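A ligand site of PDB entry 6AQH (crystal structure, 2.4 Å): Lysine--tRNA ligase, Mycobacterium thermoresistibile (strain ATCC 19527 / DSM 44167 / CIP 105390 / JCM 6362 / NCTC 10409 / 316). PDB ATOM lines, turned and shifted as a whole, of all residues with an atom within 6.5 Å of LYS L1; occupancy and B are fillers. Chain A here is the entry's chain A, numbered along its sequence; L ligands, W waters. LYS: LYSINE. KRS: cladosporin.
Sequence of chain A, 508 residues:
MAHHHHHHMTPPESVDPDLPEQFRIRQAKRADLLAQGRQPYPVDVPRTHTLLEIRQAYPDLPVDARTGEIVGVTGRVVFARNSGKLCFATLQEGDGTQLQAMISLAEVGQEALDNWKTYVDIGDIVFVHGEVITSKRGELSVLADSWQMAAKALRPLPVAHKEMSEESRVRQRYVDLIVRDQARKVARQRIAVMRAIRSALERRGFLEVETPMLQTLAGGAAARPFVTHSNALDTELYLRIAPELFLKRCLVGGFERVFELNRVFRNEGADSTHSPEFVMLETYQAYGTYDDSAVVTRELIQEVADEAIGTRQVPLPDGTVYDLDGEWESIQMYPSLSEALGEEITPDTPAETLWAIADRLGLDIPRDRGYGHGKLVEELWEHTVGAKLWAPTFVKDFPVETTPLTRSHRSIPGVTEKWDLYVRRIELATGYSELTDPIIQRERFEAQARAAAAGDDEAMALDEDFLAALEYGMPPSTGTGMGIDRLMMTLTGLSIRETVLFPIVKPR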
ATOM      1  N   GLY A 219      17.948  14.416   8.133  1.00  0.00           N
ATOM      2  CA  GLY A 219      17.271  13.220   8.598  1.00  0.00           C
ATOM      3  C   GLY A 219      16.054  12.921   7.752  1.00  0.00           C
ATOM      4  O   GLY A 219      15.838  13.521   6.708  1.00  0.00           O
ATOM      5  N   GLY A 220      15.255  11.972   8.235  1.00  0.00           N
ATOM      6  CA  GLY A 220      14.066  11.559   7.534  1.00  0.00           C
ATOM      7  C   GLY A 220      14.283  10.508   6.464  1.00  0.00           C
ATOM      8  O   GLY A 220      13.301  10.081   5.826  1.00  0.00           O
ATOM      9  N   ALA A 221      15.516  10.079   6.240  1.00  0.00           N
ATOM     10  CA  ALA A 221      15.822   9.048   5.248  1.00  0.00           C
ATOM     11  C   ALA A 221      17.205   8.494   5.556  1.00  0.00           C
ATOM     12  O   ALA A 221      17.864   8.901   6.512  1.00  0.00           O
ATOM     13  CB  ALA A 221      15.736   9.609   3.825  1.00  0.00           C
ATOM     14  N   ALA A 222      17.646   7.553   4.730  1.00  0.00           N
ATOM     15  CA  ALA A 222      18.953   6.911   4.864  1.00  0.00           C
ATOM     16  C   ALA A 222      19.793   7.272   3.647  1.00  0.00           C
ATOM     17  O   ALA A 222      19.706   6.614   2.605  1.00  0.00           O
ATOM     18  CB  ALA A 222      18.801   5.402   5.016  1.00  0.00           C
ATOM     19  N   ILE A 241      17.849  15.652   2.959  1.00  0.00           N
ATOM     20  CA  ILE A 241      17.609  14.414   2.225  1.00  0.00           C
ATOM     21  C   ILE A 241      16.149  14.011   2.227  1.00  0.00           C
ATOM     22  O   ILE A 241      15.746  13.163   1.407  1.00  0.00           O
ATOM     23  CB  ILE A 241      18.475  13.258   2.790  1.00  0.00           C
ATOM     24  CG1 ILE A 241      18.009  12.891   4.203  1.00  0.00           C
ATOM     25  CG2 ILE A 241      19.942  13.640   2.793  1.00  0.00           C
ATOM     26  CD1 ILE A 241      18.808  11.769   4.827  1.00  0.00           C
ATOM     27  N   ALA A 242      15.330  14.603   3.105  1.00  0.00           N
ATOM     28  CA  ALA A 242      13.902  14.324   3.203  1.00  0.00           C
ATOM     29  C   ALA A 242      13.264  15.376   4.094  1.00  0.00           C
ATOM     30  O   ALA A 242      13.916  15.892   5.013  1.00  0.00           O
ATOM     31  CB  ALA A 242      13.644  12.922   3.755  1.00  0.00           C
ATOM     32  N   PRO A 243      12.006  15.751   3.845  1.00  0.00           N
ATOM     33  CA  PRO A 243      11.336  16.703   4.743  1.00  0.00           C
ATOM     34  C   PRO A 243      10.517  16.020   5.826  1.00  0.00           C
ATOM     35  O   PRO A 243       9.655  16.656   6.449  1.00  0.00           O
ATOM     36  CB  PRO A 243      10.441  17.487   3.781  1.00  0.00           C
ATOM     37  CG  PRO A 243      10.049  16.459   2.766  1.00  0.00           C
ATOM     38  CD  PRO A 243      11.245  15.536   2.609  1.00  0.00           C
ATOM     39  N   GLU A 244      10.780  14.737   6.057  1.00  0.00           N
ATOM     40  CA  GLU A 244       9.934  13.930   6.925  1.00  0.00           C
ATOM     41  C   GLU A 244       9.864  14.501   8.334  1.00  0.00           C
ATOM     42  O   GLU A 244       8.777  14.647   8.911  1.00  0.00           O
ATOM     43  CB  GLU A 244      10.416  12.486   6.950  1.00  0.00           C
ATOM     44  CG  GLU A 244       9.768  11.642   8.039  1.00  0.00           C
ATOM     45  CD  GLU A 244       9.794  10.155   7.733  1.00  0.00           C
ATOM     46  OE1 GLU A 244      10.432   9.756   6.742  1.00  0.00           O
ATOM     47  OE2 GLU A 244       9.167   9.390   8.501  1.00  0.00           O
ATOM     48  N   LYS A 248       6.543  16.248  10.001  1.00  0.00           N
ATOM     49  CA  LYS A 248       5.951  15.727  11.228  1.00  0.00           C
ATOM     50  C   LYS A 248       5.750  16.828  12.261  1.00  0.00           C
ATOM     51  O   LYS A 248       4.824  16.750  13.081  1.00  0.00           O
ATOM     52  CB  LYS A 248       6.831  14.614  11.799  1.00  0.00           C
ATOM     53  CG  LYS A 248       6.327  13.271  11.275  1.00  0.00           C
ATOM     54  CD  LYS A 248       7.515  12.338  11.053  1.00  0.00           C
ATOM     55  CE  LYS A 248       7.133  10.935  11.507  1.00  0.00           C
ATOM     56  NZ  LYS A 248       7.865   9.946  10.735  1.00  0.00           N
ATOM     57  N   ARG A 266      20.584  13.989  -1.988  1.00  0.00           N
ATOM     58  CA  ARG A 266      21.231  12.831  -1.403  1.00  0.00           C
ATOM     59  C   ARG A 266      22.560  12.620  -2.128  1.00  0.00           C
ATOM     60  O   ARG A 266      22.576  12.244  -3.297  1.00  0.00           O
ATOM     61  CB  ARG A 266      20.339  11.597  -1.492  1.00  0.00           C
ATOM     62  CG  ARG A 266      18.980  11.814  -0.855  1.00  0.00           C
ATOM     63  CD  ARG A 266      18.114  10.557  -0.861  1.00  0.00           C
ATOM     64  NE  ARG A 266      16.788  10.840  -0.328  1.00  0.00           N
ATOM     65  CZ  ARG A 266      15.852   9.919  -0.103  1.00  0.00           C
ATOM     66  NH1 ARG A 266      16.095   8.640  -0.354  1.00  0.00           N
ATOM     67  NH2 ARG A 266      14.670  10.275   0.385  1.00  0.00           N
ATOM     68  N   LEU A 281       7.763  13.530  -3.419  1.00  0.00           N
ATOM     69  CA  LEU A 281       6.466  13.909  -2.880  1.00  0.00           C
ATOM     70  C   LEU A 281       6.291  13.217  -1.536  1.00  0.00           C
ATOM     71  O   LEU A 281       6.400  11.995  -1.449  1.00  0.00           O
ATOM     72  CB  LEU A 281       5.329  13.518  -3.831  1.00  0.00           C
ATOM     73  CG  LEU A 281       3.930  13.660  -3.221  1.00  0.00           C
ATOM     74  CD1 LEU A 281       3.599  15.115  -2.938  1.00  0.00           C
ATOM     75  CD2 LEU A 281       2.876  13.026  -4.110  1.00  0.00           C
ATOM     76  N   GLU A 282       6.026  14.005  -0.491  1.00  0.00           N
ATOM     77  CA  GLU A 282       5.756  13.469   0.827  1.00  0.00           C
ATOM     78  C   GLU A 282       4.427  14.033   1.319  1.00  0.00           C
ATOM     79  O   GLU A 282       4.272  15.254   1.406  1.00  0.00           O
ATOM     80  CB  GLU A 282       6.876  13.811   1.816  1.00  0.00           C
ATOM     81  CG  GLU A 282       7.977  12.767   1.883  1.00  0.00           C
ATOM     82  CD  GLU A 282       8.835  12.898   3.124  1.00  0.00           C
ATOM     83  OE1 GLU A 282      10.025  12.505   3.092  1.00  0.00           O
ATOM     84  OE2 GLU A 282       8.317  13.398   4.145  1.00  0.00           O
ATOM     85  N   THR A 283       3.485  13.147   1.624  1.00  0.00           N
ATOM     86  CA  THR A 283       2.182  13.525   2.147  1.00  0.00           C
ATOM     87  C   THR A 283       2.020  12.954   3.551  1.00  0.00           C
ATOM     88  O   THR A 283       2.594  11.913   3.884  1.00  0.00           O
ATOM     89  CB  THR A 283       1.047  12.997   1.247  1.00  0.00           C
ATOM     90  OG1 THR A 283       0.946  11.572   1.385  1.00  0.00           O
ATOM     91  CG2 THR A 283       1.315  13.332  -0.207  1.00  0.00           C
ATOM     92  N   TYR A 284       1.248  13.649   4.374  1.00  0.00           N
ATOM     93  CA  TYR A 284       0.982  13.210   5.738  1.00  0.00           C
ATOM     94  C   TYR A 284      -0.468  13.479   6.088  1.00  0.00           C
ATOM     95  O   TYR A 284      -0.948  14.615   5.934  1.00  0.00           O
ATOM     96  CB  TYR A 284       1.928  13.886   6.736  1.00  0.00           C
ATOM     97  CG  TYR A 284       3.347  13.368   6.628  1.00  0.00           C
ATOM     98  CD1 TYR A 284       4.252  13.938   5.750  1.00  0.00           C
ATOM     99  CD2 TYR A 284       3.761  12.284   7.389  1.00  0.00           C
ATOM    100  CE1 TYR A 284       5.538  13.457   5.632  1.00  0.00           C
ATOM    101  CE2 TYR A 284       5.048  11.795   7.277  1.00  0.00           C
ATOM    102  CZ  TYR A 284       5.934  12.380   6.405  1.00  0.00           C
ATOM    103  OH  TYR A 284       7.215  11.904   6.295  1.00  0.00           O
ATOM    104  N   LEU A 405      11.491   4.904  11.593  1.00  0.00           N
ATOM    105  CA  LEU A 405      10.457   5.920  11.730  1.00  0.00           C
ATOM    106  C   LEU A 405       9.062   5.367  11.536  1.00  0.00           C
ATOM    107  O   LEU A 405       8.112   6.145  11.386  1.00  0.00           O
ATOM    108  CB  LEU A 405      10.723   7.049  10.723  1.00  0.00           C
ATOM    109  CG  LEU A 405      12.093   7.705  10.808  1.00  0.00           C
ATOM    110  CD1 LEU A 405      12.308   8.683   9.657  1.00  0.00           C
ATOM    111  CD2 LEU A 405      12.283   8.393  12.144  1.00  0.00           C
ATOM    112  N   THR A 430       6.455   4.757  -0.993  1.00  0.00           N
ATOM    113  CA  THR A 430       6.442   4.071   0.296  1.00  0.00           C
ATOM    114  C   THR A 430       5.455   4.780   1.210  1.00  0.00           C
ATOM    115  O   THR A 430       5.067   5.928   0.970  1.00  0.00           O
ATOM    116  CB  THR A 430       7.839   4.045   0.942  1.00  0.00           C
ATOM    117  OG1 THR A 430       7.772   3.311   2.177  1.00  0.00           O
ATOM    118  CG2 THR A 430       8.320   5.454   1.222  1.00  0.00           C
ATOM    119  N   GLY A 431       5.044   4.087   2.257  1.00  0.00           N
ATOM    120  CA  GLY A 431       4.093   4.647   3.199  1.00  0.00           C
ATOM    121  C   GLY A 431       4.136   4.004   4.572  1.00  0.00           C
ATOM    122  O   GLY A 431       4.175   2.774   4.677  1.00  0.00           O
ATOM    123  N   TYR A 432       4.126   4.821   5.626  1.00  0.00           N
ATOM    124  CA  TYR A 432       4.201   4.339   6.990  1.00  0.00           C
ATOM    125  C   TYR A 432       2.917   4.675   7.739  1.00  0.00           C
ATOM    126  O   TYR A 432       2.232   5.659   7.433  1.00  0.00           O
ATOM    127  CB  TYR A 432       5.370   4.964   7.778  1.00  0.00           C
ATOM    128  CG  TYR A 432       6.734   4.911   7.142  1.00  0.00           C
ATOM    129  CD1 TYR A 432       7.044   3.989   6.146  1.00  0.00           C
ATOM    130  CD2 TYR A 432       7.731   5.787   7.557  1.00  0.00           C
ATOM    131  CE1 TYR A 432       8.306   3.970   5.575  1.00  0.00           C
ATOM    132  CE2 TYR A 432       8.993   5.760   6.991  1.00  0.00           C
ATOM    133  CZ  TYR A 432       9.272   4.855   6.006  1.00  0.00           C
ATOM    134  OH  TYR A 432      10.535   4.827   5.440  1.00  0.00           O
ATOM    135  N   GLU A 434       2.722   6.260  10.964  1.00  0.00           N
ATOM    136  CA  GLU A 434       3.802   7.008  11.579  1.00  0.00           C
ATOM    137  C   GLU A 434       3.978   6.641  13.046  1.00  0.00           C
ATOM    138  O   GLU A 434       3.010   6.522  13.801  1.00  0.00           O
ATOM    139  CB  GLU A 434       3.554   8.504  11.430  1.00  0.00           C
ATOM    140  CG  GLU A 434       3.483   8.981   9.991  1.00  0.00           C
ATOM    141  CD  GLU A 434       4.739   8.670   9.196  1.00  0.00           C
ATOM    142  OE1 GLU A 434       5.841   8.634   9.796  1.00  0.00           O
ATOM    143  OE2 GLU A 434       4.636   8.452   7.972  1.00  0.00           O
ATOM    144  N   THR A 478      -0.606   8.775   9.021  1.00  0.00           N
ATOM    145  CA  THR A 478       0.117   8.021   8.008  1.00  0.00           C
ATOM    146  C   THR A 478       0.800   8.987   7.045  1.00  0.00           C
ATOM    147  O   THR A 478       0.284  10.071   6.759  1.00  0.00           O
ATOM    148  CB  THR A 478      -0.815   7.085   7.231  1.00  0.00           C
ATOM    149  OG1 THR A 478      -0.089   6.435   6.190  1.00  0.00           O
ATOM    150  CG2 THR A 478      -1.981   7.858   6.624  1.00  0.00           C
ATOM    151  N   GLY A 479       1.964   8.584   6.564  1.00  0.00           N
ATOM    152  CA  GLY A 479       2.729   9.409   5.650  1.00  0.00           C
ATOM    153  C   GLY A 479       3.229   8.598   4.465  1.00  0.00           C
ATOM    154  O   GLY A 479       3.440   7.394   4.559  1.00  0.00           O
ATOM    155  N   THR A 480       3.415   9.297   3.349  1.00  0.00           N
ATOM    156  CA  THR A 480       3.883   8.671   2.115  1.00  0.00           C
ATOM    157  C   THR A 480       5.105   9.402   1.584  1.00  0.00           C
ATOM    158  O   THR A 480       5.364  10.558   1.916  1.00  0.00           O
ATOM    159  CB  THR A 480       2.792   8.663   1.030  1.00  0.00           C
ATOM    160  OG1 THR A 480       2.469  10.014   0.666  1.00  0.00           O
ATOM    161  CG2 THR A 480       1.543   7.970   1.534  1.00  0.00           C
ATOM    162  N   GLY A 481       5.854   8.700   0.739  1.00  0.00           N
ATOM    163  CA  GLY A 481       6.963   9.275   0.017  1.00  0.00           C
ATOM    164  C   GLY A 481       7.009   8.710  -1.396  1.00  0.00           C
ATOM    165  O   GLY A 481       6.759   7.517  -1.578  1.00  0.00           O
ATOM    166  N   MET A 482       7.314   9.545  -2.386  1.00  0.00           N
ATOM    167  CA  MET A 482       7.331   9.087  -3.767  1.00  0.00           C
ATOM    168  C   MET A 482       8.286   9.940  -4.576  1.00  0.00           C
ATOM    169  O   MET A 482       8.217  11.179  -4.531  1.00  0.00           O
ATOM    170  CB  MET A 482       5.931   9.132  -4.387  1.00  0.00           C
ATOM    171  CG  MET A 482       5.879   8.645  -5.830  1.00  0.00           C
ATOM    172  SD  MET A 482       4.212   8.593  -6.516  1.00  0.00           S
ATOM    173  CE  MET A 482       3.805  10.339  -6.536  1.00  0.00           C
HETATM  174  N   LYS L   1      11.125  10.069   4.337  1.00  0.00           N
HETATM  175  CA  LYS L   1      10.782   8.950   3.478  1.00  0.00           C
HETATM  176  C   LYS L   1      11.904   8.718   2.458  1.00  0.00           C
HETATM  177  O   LYS L   1      12.680   9.658   2.154  1.00  0.00           O
HETATM  178  CB  LYS L   1       9.457   9.207   2.760  1.00  0.00           C
HETATM  179  CG  LYS L   1       8.323   9.317   3.786  1.00  0.00           C
HETATM  180  CD  LYS L   1       7.953   7.928   4.291  1.00  0.00           C
HETATM  181  CE  LYS L   1       6.648   7.996   5.072  1.00  0.00           C
HETATM  182  NZ  LYS L   1       6.865   8.682   6.332  1.00  0.00           N
HETATM  183  OXT LYS L   1      12.038   7.589   1.924  1.00  0.00           O
HETATM  184  O4  KRS L   2      14.564   8.561  -7.201  1.00  0.00           O
HETATM  185  C8  KRS L   2      14.933   8.207  -6.124  1.00  0.00           C
HETATM  186  C9  KRS L   2      16.258   8.465  -5.521  1.00  0.00           C
HETATM  187  C5  KRS L   2      16.594   7.938  -4.281  1.00  0.00           C
HETATM  188  C4  KRS L   2      17.837   8.181  -3.717  1.00  0.00           C
HETATM  189  C3  KRS L   2      18.753   8.955  -4.389  1.00  0.00           C
HETATM  190  O2  KRS L   2      19.997   9.232  -3.899  1.00  0.00           O
HETATM  191  C2  KRS L   2      18.436   9.489  -5.623  1.00  0.00           C
HETATM  192  C1  KRS L   2      17.201   9.257  -6.190  1.00  0.00           C
HETATM  193  O1  KRS L   2      16.878   9.777  -7.391  1.00  0.00           O
HETATM  194  O3  KRS L   2      14.045   7.501  -5.347  1.00  0.00           O
HETATM  195  C7  KRS L   2      14.157   7.419  -3.906  1.00  0.00           C
HETATM  196  C6  KRS L   2      15.596   7.073  -3.530  1.00  0.00           C
HETATM  197  C10 KRS L   2      13.158   6.427  -3.311  1.00  0.00           C
HETATM  198  C11 KRS L   2      11.694   6.706  -3.670  1.00  0.00           C
HETATM  199  O5  KRS L   2      11.476   8.072  -3.222  1.00  0.00           O
HETATM  200  C12 KRS L   2      11.464   8.326  -1.796  1.00  0.00           C
HETATM  201  C16 KRS L   2      11.156   9.796  -1.496  1.00  0.00           C
HETATM  202  C13 KRS L   2      10.504   7.358  -1.074  1.00  0.00           C
HETATM  203  C14 KRS L   2       9.729   6.508  -2.084  1.00  0.00           C
HETATM  204  C15 KRS L   2      10.702   5.746  -2.999  1.00  0.00           C
HETATM  205  O   HOH W   1      11.724  12.432   0.797  1.00  0.00           O
HETATM  206  O   HOH W   2      11.653   5.152   2.688  1.00  0.00           O
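N of LYS L1 sits at hydrogen-bond distance from O of Gly 220 (2.6 Å).
The guanidinium group (NH2) of Arg 266 is in salt-bridge range of an oxygen (O) of LYS L1 (2.7 Å).
A nitrogen (N) of LYS L1 lies within salt-bridge range of the side-chain carboxylate (OE1) of Glu 244.
OE1 of Glu 282 lies within salt-bridge range of N of LYS L1 (2.9 Å).
The side-chain hydroxyl (OH) of Tyr 284 lies within hydrogen-bond range of a nitrogen (NZ) of LYS L1 (3.2 Å).
The side-chain carboxylate of Glu 434 is in salt-bridge range of a nitrogen (NZ) of LYS L1, 2.8 Å away.
OG1 of Thr 478 is in hydrogen-bond range of O of Tyr 432, 2.7 Å away.
The backbone NH (N) of Tyr 432 lies within hydrogen-bond range of the backbone carbonyl oxygen (O) of Gly 479.
The side-chain carboxylate (OE1) of Glu 434 is in salt-bridge range of the side-chain amino group (NZ) of Lys 248 (2.6 Å).
The backbone NH (N) of Thr 480 is in hydrogen-bond range of the backbone carbonyl oxygen (O) of Thr 283 (2.8 Å).
The backbone carbonyl oxygen (O) of Gly 481 sits at hydrogen-bond distance from the backbone NH (N) of Thr 430, 2.8 Å away.
The side-chain carboxylate (OE2) of Glu 434 is in hydrogen-bond range of the backbone NH (N) of Gly 479.
The backbone carbonyl oxygen of Ile 241 is in hydrogen-bond range of the guanidinium group of Arg 266 (3.1 Å).
The side-chain carboxylate (OE2) of Glu 282 sits at hydrogen-bond distance from the side-chain hydroxyl (OH) of Tyr 284.
Merely in contact with LYS L1: Ala 221 (3.5 Å), Ala 242 (3.8 Å), Thr 430 (3.96 Å), Tyr 432 (3.3 Å), Gly 479 (3.3 Å), Thr 480 (3.7 Å) and Gly 481 (3.7 Å).
Hydrophobic or aromatic side chains within 4 Å of LYS L1: Ala 221, Ala 242, Tyr 284 and Tyr 432.
Of the 24 residues printed, 13 come within 4 Å of LYS L1.
Water W2 bridges an oxygen (OXT) of LYS L1 (2.6 Å) and the side-chain hydroxyl of Tyr 432 (3.0 Å).
Water W1 lies within hydrogen-bond range of the side-chain carboxylate of Glu 282 (2.9 Å) and an oxygen (O) of LYS L1 (3.2 Å).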
